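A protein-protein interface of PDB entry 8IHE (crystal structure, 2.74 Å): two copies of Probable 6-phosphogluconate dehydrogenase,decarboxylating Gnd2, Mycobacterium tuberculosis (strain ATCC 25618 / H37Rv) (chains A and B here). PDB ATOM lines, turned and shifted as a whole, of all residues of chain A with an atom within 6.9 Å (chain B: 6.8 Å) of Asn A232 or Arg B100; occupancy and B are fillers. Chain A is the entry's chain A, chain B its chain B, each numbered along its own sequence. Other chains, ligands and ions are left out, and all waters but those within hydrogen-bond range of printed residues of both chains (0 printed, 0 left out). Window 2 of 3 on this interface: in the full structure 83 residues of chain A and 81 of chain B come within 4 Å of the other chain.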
ATOM      1  N   GLY A 217      11.232 -10.831 -17.080  1.00  0.00           N
ATOM      2  CA  GLY A 217      11.942 -10.945 -15.785  1.00  0.00           C
ATOM      3  C   GLY A 217      13.413 -10.554 -15.886  1.00  0.00           C
ATOM      4  O   GLY A 217      14.092 -10.514 -14.844  1.00  0.00           O
ATOM      5  N   LEU A 230       7.076  -6.707 -10.537  1.00  0.00           N
ATOM      6  CA  LEU A 230       6.914  -8.131 -10.949  1.00  0.00           C
ATOM      7  C   LEU A 230       7.406  -9.051  -9.834  1.00  0.00           C
ATOM      8  O   LEU A 230       8.614  -9.191  -9.639  1.00  0.00           O
ATOM      9  CB  LEU A 230       7.689  -8.406 -12.245  1.00  0.00           C
ATOM     10  CG  LEU A 230       7.586  -9.837 -12.779  1.00  0.00           C
ATOM     11  CD1 LEU A 230       6.143 -10.199 -13.093  1.00  0.00           C
ATOM     12  CD2 LEU A 230       8.462 -10.020 -14.005  1.00  0.00           C
ATOM     13  N   PRO A 231       6.506  -9.738  -9.092  1.00  0.00           N
ATOM     14  CA  PRO A 231       6.952 -10.755  -8.146  1.00  0.00           C
ATOM     15  C   PRO A 231       7.616 -11.905  -8.922  1.00  0.00           C
ATOM     16  O   PRO A 231       7.147 -12.275 -10.007  1.00  0.00           O
ATOM     17  CB  PRO A 231       5.670 -11.173  -7.407  1.00  0.00           C
ATOM     18  CG  PRO A 231       4.550 -10.834  -8.378  1.00  0.00           C
ATOM     19  CD  PRO A 231       5.037  -9.612  -9.132  1.00  0.00           C
ATOM     20  N   ASN A 232       8.727 -12.403  -8.381  1.00  0.00           N
ATOM     21  CA  ASN A 232       9.367 -13.670  -8.819  1.00  0.00           C
ATOM     22  C   ASN A 232       9.802 -13.549 -10.285  1.00  0.00           C
ATOM     23  O   ASN A 232       9.424 -14.385 -11.108  1.00  0.00           O
ATOM     24  CB  ASN A 232       8.410 -14.840  -8.548  1.00  0.00           C
ATOM     25  CG  ASN A 232       7.555 -14.640  -7.307  1.00  0.00           C
ATOM     26  OD1 ASN A 232       8.069 -14.329  -6.233  1.00  0.00           O
ATOM     27  ND2 ASN A 232       6.246 -14.801  -7.438  1.00  0.00           N
ATOM     28  N   PRO A 233      10.634 -12.537 -10.656  1.00  0.00           N
ATOM     29  CA  PRO A 233      11.063 -12.339 -12.043  1.00  0.00           C
ATOM     30  C   PRO A 233      12.120 -13.355 -12.496  1.00  0.00           C
ATOM     31  O   PRO A 233      12.472 -13.341 -13.653  1.00  0.00           O
ATOM     32  CB  PRO A 233      11.652 -10.922 -12.040  1.00  0.00           C
ATOM     33  CG  PRO A 233      12.203 -10.778 -10.651  1.00  0.00           C
ATOM     34  CD  PRO A 233      11.238 -11.537  -9.761  1.00  0.00           C
ATOM     35  N   GLU A 234      12.602 -14.193 -11.577  1.00  0.00           N
ATOM     36  CA  GLU A 234      13.396 -15.409 -11.898  1.00  0.00           C
ATOM     37  C   GLU A 234      12.528 -16.355 -12.746  1.00  0.00           C
ATOM     38  O   GLU A 234      13.092 -17.127 -13.567  1.00  0.00           O
ATOM     39  CB  GLU A 234      13.910 -16.067 -10.609  1.00  0.00           C
ATOM     40  CG  GLU A 234      12.837 -16.706  -9.724  1.00  0.00           C
ATOM     41  CD  GLU A 234      12.314 -15.877  -8.557  1.00  0.00           C
ATOM     42  OE1 GLU A 234      11.724 -16.482  -7.636  1.00  0.00           O
ATOM     43  OE2 GLU A 234      12.488 -14.635  -8.562  1.00  0.00           O
ATOM     44  N   CYS A 235      11.206 -16.280 -12.555  1.00  0.00           N
ATOM     45  CA  CYS A 235      10.191 -17.135 -13.224  1.00  0.00           C
ATOM     46  C   CYS A 235      10.126 -16.793 -14.721  1.00  0.00           C
ATOM     47  O   CYS A 235      10.122 -17.730 -15.545  1.00  0.00           O
ATOM     48  CB  CYS A 235       8.847 -16.987 -12.524  1.00  0.00           C
ATOM     49  SG  CYS A 235       8.919 -17.482 -10.779  1.00  0.00           S
ATOM     50  N   TYR A 236      10.150 -15.504 -15.065  1.00  0.00           N
ATOM     51  CA  TYR A 236       9.946 -15.018 -16.453  1.00  0.00           C
ATOM     52  C   TYR A 236      11.293 -14.677 -17.115  1.00  0.00           C
ATOM     53  O   TYR A 236      11.514 -13.507 -17.500  1.00  0.00           O
ATOM     54  CB  TYR A 236       8.959 -13.845 -16.445  1.00  0.00           C
ATOM     55  CG  TYR A 236       7.604 -14.157 -15.858  1.00  0.00           C
ATOM     56  CD1 TYR A 236       6.704 -14.973 -16.522  1.00  0.00           C
ATOM     57  CD2 TYR A 236       7.225 -13.642 -14.627  1.00  0.00           C
ATOM     58  CE1 TYR A 236       5.465 -15.272 -15.983  1.00  0.00           C
ATOM     59  CE2 TYR A 236       5.989 -13.936 -14.067  1.00  0.00           C
ATOM     60  CZ  TYR A 236       5.099 -14.749 -14.751  1.00  0.00           C
ATOM     61  OH  TYR A 236       3.881 -15.028 -14.198  1.00  0.00           O
ATOM     62  N   TYR A 238      12.517 -16.602 -19.981  1.00  0.00           N
ATOM     63  CA  TYR A 238      12.510 -17.432 -21.211  1.00  0.00           C
ATOM     64  C   TYR A 238      12.496 -16.558 -22.473  1.00  0.00           C
ATOM     65  O   TYR A 238      11.653 -15.650 -22.558  1.00  0.00           O
ATOM     66  CB  TYR A 238      11.317 -18.372 -21.184  1.00  0.00           C
ATOM     67  CG  TYR A 238      11.267 -19.263 -19.973  1.00  0.00           C
ATOM     68  CD1 TYR A 238      12.339 -20.072 -19.632  1.00  0.00           C
ATOM     69  CD2 TYR A 238      10.134 -19.334 -19.182  1.00  0.00           C
ATOM     70  CE1 TYR A 238      12.292 -20.924 -18.536  1.00  0.00           C
ATOM     71  CE2 TYR A 238      10.081 -20.164 -18.073  1.00  0.00           C
ATOM     72  CZ  TYR A 238      11.163 -20.961 -17.743  1.00  0.00           C
ATOM     73  OH  TYR A 238      11.099 -21.772 -16.647  1.00  0.00           O
ATOM     74  N   THR B  97       3.283 -30.726 -14.724  1.00  0.00           N
ATOM     75  CA  THR B  97       3.938 -30.005 -13.594  1.00  0.00           C
ATOM     76  C   THR B  97       3.928 -28.508 -13.912  1.00  0.00           C
ATOM     77  O   THR B  97       4.416 -28.166 -14.983  1.00  0.00           O
ATOM     78  CB  THR B  97       5.393 -30.472 -13.370  1.00  0.00           C
ATOM     79  OG1 THR B  97       5.503 -31.871 -13.104  1.00  0.00           O
ATOM     80  CG2 THR B  97       6.063 -29.738 -12.227  1.00  0.00           C
ATOM     81  N   TYR B  98       3.425 -27.659 -13.014  1.00  0.00           N
ATOM     82  CA  TYR B  98       3.673 -26.193 -13.042  1.00  0.00           C
ATOM     83  C   TYR B  98       5.187 -25.980 -13.213  1.00  0.00           C
ATOM     84  O   TYR B  98       5.965 -26.495 -12.376  1.00  0.00           O
ATOM     85  CB  TYR B  98       3.187 -25.521 -11.760  1.00  0.00           C
ATOM     86  CG  TYR B  98       3.114 -24.010 -11.745  1.00  0.00           C
ATOM     87  CD1 TYR B  98       2.995 -23.245 -12.897  1.00  0.00           C
ATOM     88  CD2 TYR B  98       3.085 -23.330 -10.535  1.00  0.00           C
ATOM     89  CE1 TYR B  98       2.891 -21.857 -12.847  1.00  0.00           C
ATOM     90  CE2 TYR B  98       2.974 -21.949 -10.465  1.00  0.00           C
ATOM     91  CZ  TYR B  98       2.864 -21.202 -11.625  1.00  0.00           C
ATOM     92  OH  TYR B  98       2.716 -19.843 -11.540  1.00  0.00           O
ATOM     93  N   TYR B  99       5.594 -25.277 -14.277  1.00  0.00           N
ATOM     94  CA  TYR B  99       7.007 -24.946 -14.580  1.00  0.00           C
ATOM     95  C   TYR B  99       7.680 -24.375 -13.320  1.00  0.00           C
ATOM     96  O   TYR B  99       8.846 -24.671 -13.091  1.00  0.00           O
ATOM     97  CB  TYR B  99       7.106 -24.006 -15.788  1.00  0.00           C
ATOM     98  CG  TYR B  99       6.884 -22.545 -15.498  1.00  0.00           C
ATOM     99  CD1 TYR B  99       5.604 -22.021 -15.422  1.00  0.00           C
ATOM    100  CD2 TYR B  99       7.952 -21.685 -15.298  1.00  0.00           C
ATOM    101  CE1 TYR B  99       5.396 -20.678 -15.164  1.00  0.00           C
ATOM    102  CE2 TYR B  99       7.754 -20.344 -15.020  1.00  0.00           C
ATOM    103  CZ  TYR B  99       6.473 -19.835 -14.960  1.00  0.00           C
ATOM    104  OH  TYR B  99       6.259 -18.507 -14.717  1.00  0.00           O
ATOM    105  N   ARG B 100       6.989 -23.592 -12.495  1.00  0.00           N
ATOM    106  CA  ARG B 100       7.636 -23.021 -11.275  1.00  0.00           C
ATOM    107  C   ARG B 100       8.191 -24.190 -10.423  1.00  0.00           C
ATOM    108  O   ARG B 100       9.317 -24.069  -9.928  1.00  0.00           O
ATOM    109  CB  ARG B 100       6.694 -22.054 -10.536  1.00  0.00           C
ATOM    110  CG  ARG B 100       6.401 -20.760 -11.288  1.00  0.00           C
ATOM    111  CD  ARG B 100       5.978 -19.587 -10.405  1.00  0.00           C
ATOM    112  NE  ARG B 100       5.131 -18.586 -11.064  1.00  0.00           N
ATOM    113  CZ  ARG B 100       4.759 -17.414 -10.532  1.00  0.00           C
ATOM    114  NH1 ARG B 100       5.184 -17.037  -9.340  1.00  0.00           N
ATOM    115  NH2 ARG B 100       3.964 -16.594 -11.198  1.00  0.00           N
ATOM    116  N   ASP B 101       7.475 -25.313 -10.325  1.00  0.00           N
ATOM    117  CA  ASP B 101       7.851 -26.477  -9.479  1.00  0.00           C
ATOM    118  C   ASP B 101       8.973 -27.243 -10.179  1.00  0.00           C
ATOM    119  O   ASP B 101       9.707 -27.962  -9.499  1.00  0.00           O
ATOM    120  CB  ASP B 101       6.649 -27.376  -9.177  1.00  0.00           C
ATOM    121  CG  ASP B 101       5.618 -26.761  -8.234  1.00  0.00           C
ATOM    122  OD1 ASP B 101       5.955 -25.773  -7.538  1.00  0.00           O
ATOM    123  OD2 ASP B 101       4.470 -27.266  -8.203  1.00  0.00           O
ATOM    124  N   ASP B 102       9.124 -27.076 -11.488  1.00  0.00           N
ATOM    125  CA  ASP B 102      10.272 -27.647 -12.237  1.00  0.00           C
ATOM    126  C   ASP B 102      11.577 -27.030 -11.707  1.00  0.00           C
ATOM    127  O   ASP B 102      12.547 -27.789 -11.534  1.00  0.00           O
ATOM    128  CB  ASP B 102      10.108 -27.483 -13.753  1.00  0.00           C
ATOM    129  CG  ASP B 102       9.331 -28.609 -14.420  1.00  0.00           C
ATOM    130  OD1 ASP B 102       9.275 -29.723 -13.842  1.00  0.00           O
ATOM    131  OD2 ASP B 102       8.795 -28.369 -15.514  1.00  0.00           O
ATOM    132  N   LEU B 103      11.613 -25.720 -11.438  1.00  0.00           N
ATOM    133  CA  LEU B 103      12.849 -25.022 -10.974  1.00  0.00           C
ATOM    134  C   LEU B 103      13.291 -25.648  -9.640  1.00  0.00           C
ATOM    135  O   LEU B 103      14.474 -26.076  -9.539  1.00  0.00           O
ATOM    136  CB  LEU B 103      12.597 -23.508 -10.866  1.00  0.00           C
ATOM    137  CG  LEU B 103      12.371 -22.789 -12.200  1.00  0.00           C
ATOM    138  CD1 LEU B 103      12.470 -21.286 -12.042  1.00  0.00           C
ATOM    139  CD2 LEU B 103      13.345 -23.273 -13.264  1.00  0.00           C
ATOM    140  N   ARG B 104      12.353 -25.758  -8.690  1.00  0.00           N
ATOM    141  CA  ARG B 104      12.545 -26.417  -7.371  1.00  0.00           C
ATOM    142  C   ARG B 104      13.050 -27.852  -7.582  1.00  0.00           C
ATOM    143  O   ARG B 104      14.075 -28.210  -6.991  1.00  0.00           O
ATOM    144  CB  ARG B 104      11.239 -26.371  -6.577  1.00  0.00           C
ATOM    145  CG  ARG B 104      10.926 -25.003  -5.987  1.00  0.00           C
ATOM    146  CD  ARG B 104       9.504 -24.880  -5.462  1.00  0.00           C
ATOM    147  NE  ARG B 104       9.082 -26.083  -4.753  1.00  0.00           N
ATOM    148  CZ  ARG B 104       7.821 -26.444  -4.545  1.00  0.00           C
ATOM    149  NH1 ARG B 104       6.822 -25.690  -4.980  1.00  0.00           N
ATOM    150  NH2 ARG B 104       7.560 -27.566  -3.896  1.00  0.00           N
ATOM    151  N   HIS B 105      12.382 -28.636  -8.428  1.00  0.00           N
ATOM    152  CA  HIS B 105      12.752 -30.042  -8.732  1.00  0.00           C
ATOM    153  C   HIS B 105      14.157 -30.128  -9.333  1.00  0.00           C
ATOM    154  O   HIS B 105      14.731 -31.212  -9.303  1.00  0.00           O
ATOM    155  CB  HIS B 105      11.740 -30.682  -9.690  1.00  0.00           C
ATOM    156  CG  HIS B 105      10.456 -31.048  -9.026  1.00  0.00           C
ATOM    157  ND1 HIS B 105       9.686 -32.120  -9.445  1.00  0.00           N
ATOM    158  CD2 HIS B 105       9.826 -30.509  -7.958  1.00  0.00           C
ATOM    159  CE1 HIS B 105       8.620 -32.205  -8.678  1.00  0.00           C
ATOM    160  NE2 HIS B 105       8.681 -31.218  -7.756  1.00  0.00           N
ATOM    161  N   GLY B 184      11.996 -25.861 -17.180  1.00  0.00           N
ATOM    162  CA  GLY B 184      10.665 -25.216 -17.156  1.00  0.00           C
ATOM    163  C   GLY B 184      10.134 -24.915 -18.557  1.00  0.00           C
ATOM    164  O   GLY B 184       9.089 -25.489 -18.948  1.00  0.00           O
ATOM    165  N   TRP B 288      -2.587 -21.065 -15.140  1.00  0.00           N
ATOM    166  CA  TRP B 288      -1.155 -20.650 -15.024  1.00  0.00           C
ATOM    167  C   TRP B 288      -0.792 -19.739 -16.206  1.00  0.00           C
ATOM    168  O   TRP B 288      -0.039 -18.723 -15.972  1.00  0.00           O
ATOM    169  CB  TRP B 288      -0.193 -21.854 -14.910  1.00  0.00           C
ATOM    170  CG  TRP B 288      -0.525 -22.798 -13.782  1.00  0.00           C
ATOM    171  CD1 TRP B 288      -1.123 -22.485 -12.591  1.00  0.00           C
ATOM    172  CD2 TRP B 288      -0.333 -24.227 -13.760  1.00  0.00           C
ATOM    173  NE1 TRP B 288      -1.336 -23.616 -11.846  1.00  0.00           N
ATOM    174  CE2 TRP B 288      -0.840 -24.697 -12.529  1.00  0.00           C
ATOM    175  CE3 TRP B 288       0.201 -25.158 -14.662  1.00  0.00           C
ATOM    176  CZ2 TRP B 288      -0.808 -26.046 -12.179  1.00  0.00           C
ATOM    177  CZ3 TRP B 288       0.243 -26.497 -14.314  1.00  0.00           C
ATOM    178  CH2 TRP B 288      -0.264 -26.929 -13.085  1.00  0.00           C
ATOM    179  N   ILE B 291      -2.307 -16.331 -15.570  1.00  0.00           N
ATOM    180  CA  ILE B 291      -1.414 -15.685 -14.561  1.00  0.00           C
ATOM    181  C   ILE B 291      -0.135 -15.244 -15.271  1.00  0.00           C
ATOM    182  O   ILE B 291       0.242 -14.072 -15.159  1.00  0.00           O
ATOM    183  CB  ILE B 291      -1.138 -16.600 -13.350  1.00  0.00           C
ATOM    184  CG1 ILE B 291      -2.402 -16.853 -12.505  1.00  0.00           C
ATOM    185  CG2 ILE B 291      -0.020 -16.023 -12.495  1.00  0.00           C
ATOM    186  CD1 ILE B 291      -2.347 -18.105 -11.632  1.00  0.00           C
ATOM    187  N   ALA B 292       0.478 -16.108 -16.066  1.00  0.00           N
ATOM    188  CA  ALA B 292       1.645 -15.695 -16.871  1.00  0.00           C
ATOM    189  C   ALA B 292       1.260 -14.430 -17.630  1.00  0.00           C
ATOM    190  O   ALA B 292       2.050 -13.508 -17.651  1.00  0.00           O
ATOM    191  CB  ALA B 292       2.064 -16.807 -17.789  1.00  0.00           C
ATOM    192  N   ASP B 295       0.824 -11.182 -15.311  1.00  0.00           N
ATOM    193  CA  ASP B 295       2.136 -10.769 -14.776  1.00  0.00           C
ATOM    194  C   ASP B 295       2.981 -10.058 -15.832  1.00  0.00           C
ATOM    195  O   ASP B 295       3.776  -9.233 -15.408  1.00  0.00           O
ATOM    196  CB  ASP B 295       2.958 -11.971 -14.314  1.00  0.00           C
ATOM    197  CG  ASP B 295       2.710 -12.388 -12.886  1.00  0.00           C
ATOM    198  OD1 ASP B 295       2.293 -11.498 -12.072  1.00  0.00           O
ATOM    199  OD2 ASP B 295       2.947 -13.590 -12.616  1.00  0.00           O
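ND2 of Asn A232 lies close to NH1 of Arg B100, at 3.1 Å. The side-chain hydroxyl of Tyr A236 is in hydrogen-bond range of the guanidinium group of Arg B100 (3.4 Å). OH of Tyr A236 sits close to OD2 of Asp B295 (2.3 Å).
Of chain A, only Asn A232, Cys A235 and Tyr A236 come within 4 Å of Arg B100. Printed residues of chain B within 4 Å of Leu A230: Asp B295. Printed residues of chain A within 4 Å of Asp B295: Leu A230 (3.4 Å) and Tyr A236 (2.3 Å). Of the printed residues of chain B, Tyr A236 touches Tyr B99, Arg B100, Ile B291, Ala B292 and Asp B295. Thr B97 touches none of the printed residues of chain A. His B105 touches none of the printed residues of chain A. The nearest residue of chain A that does not touch Arg B100 is Pro A231 (5.2 Å).
Asp B295 touches Leu A230 (O to CD1, 3.4 Å). Cys A235 touches Tyr B99. Arg B100 touches Cys A235. Tyr A236 touches Tyr B99. Tyr A236 touches Ile B291 (OH to O, 3.9 Å). OH of Tyr A236 touches CA of Ala B292, 3.5 Å away. OH of Tyr A238 touches CD2 of Tyr B99 (3.4 Å). CA of Gly B184 touches OH of Tyr A238, 3.5 Å away.
No position is printed for both chains. Of the 11 pairs that touch across the chains among the printed residues, none has its exchanged pair printed and touching as well.
Printed residues of chain B that touch a printed residue of chain A: Tyr B99, Arg B100, Gly B184, Ile B291, Ala B292 and Asp B295. Hydrophobic or aromatic side chains of chain B within 4 Å of the printed part of chain A: Tyr B99. Of the 9 printed residues of chain A, 5 touch a printed residue of chain B. Hydrophobic or aromatic side chains of chain A that line the printed part of chain B: Leu A230, Tyr A236 and Tyr A238. Among the printed residues, no Asp or Glu carboxylate lies within 4 Å of a Lys or Arg side-chain nitrogen of the other chain.
The backbone NH (N) of Gly A217 sits at hydrogen-bond distance from the backbone carbonyl oxygen (O) of Tyr A236 (2.7 Å). O of Asn A232 lies close to SG of Cys A235 (3.2 Å). The side-chain hydroxyl (OH) of Tyr B98 lies within hydrogen-bond range of the guanidinium group (NE) of Arg B100, at 2.8 Å. OD2 of Asp B295 lies within salt-bridge range of NH2 of Arg B100, at 3.5 Å.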
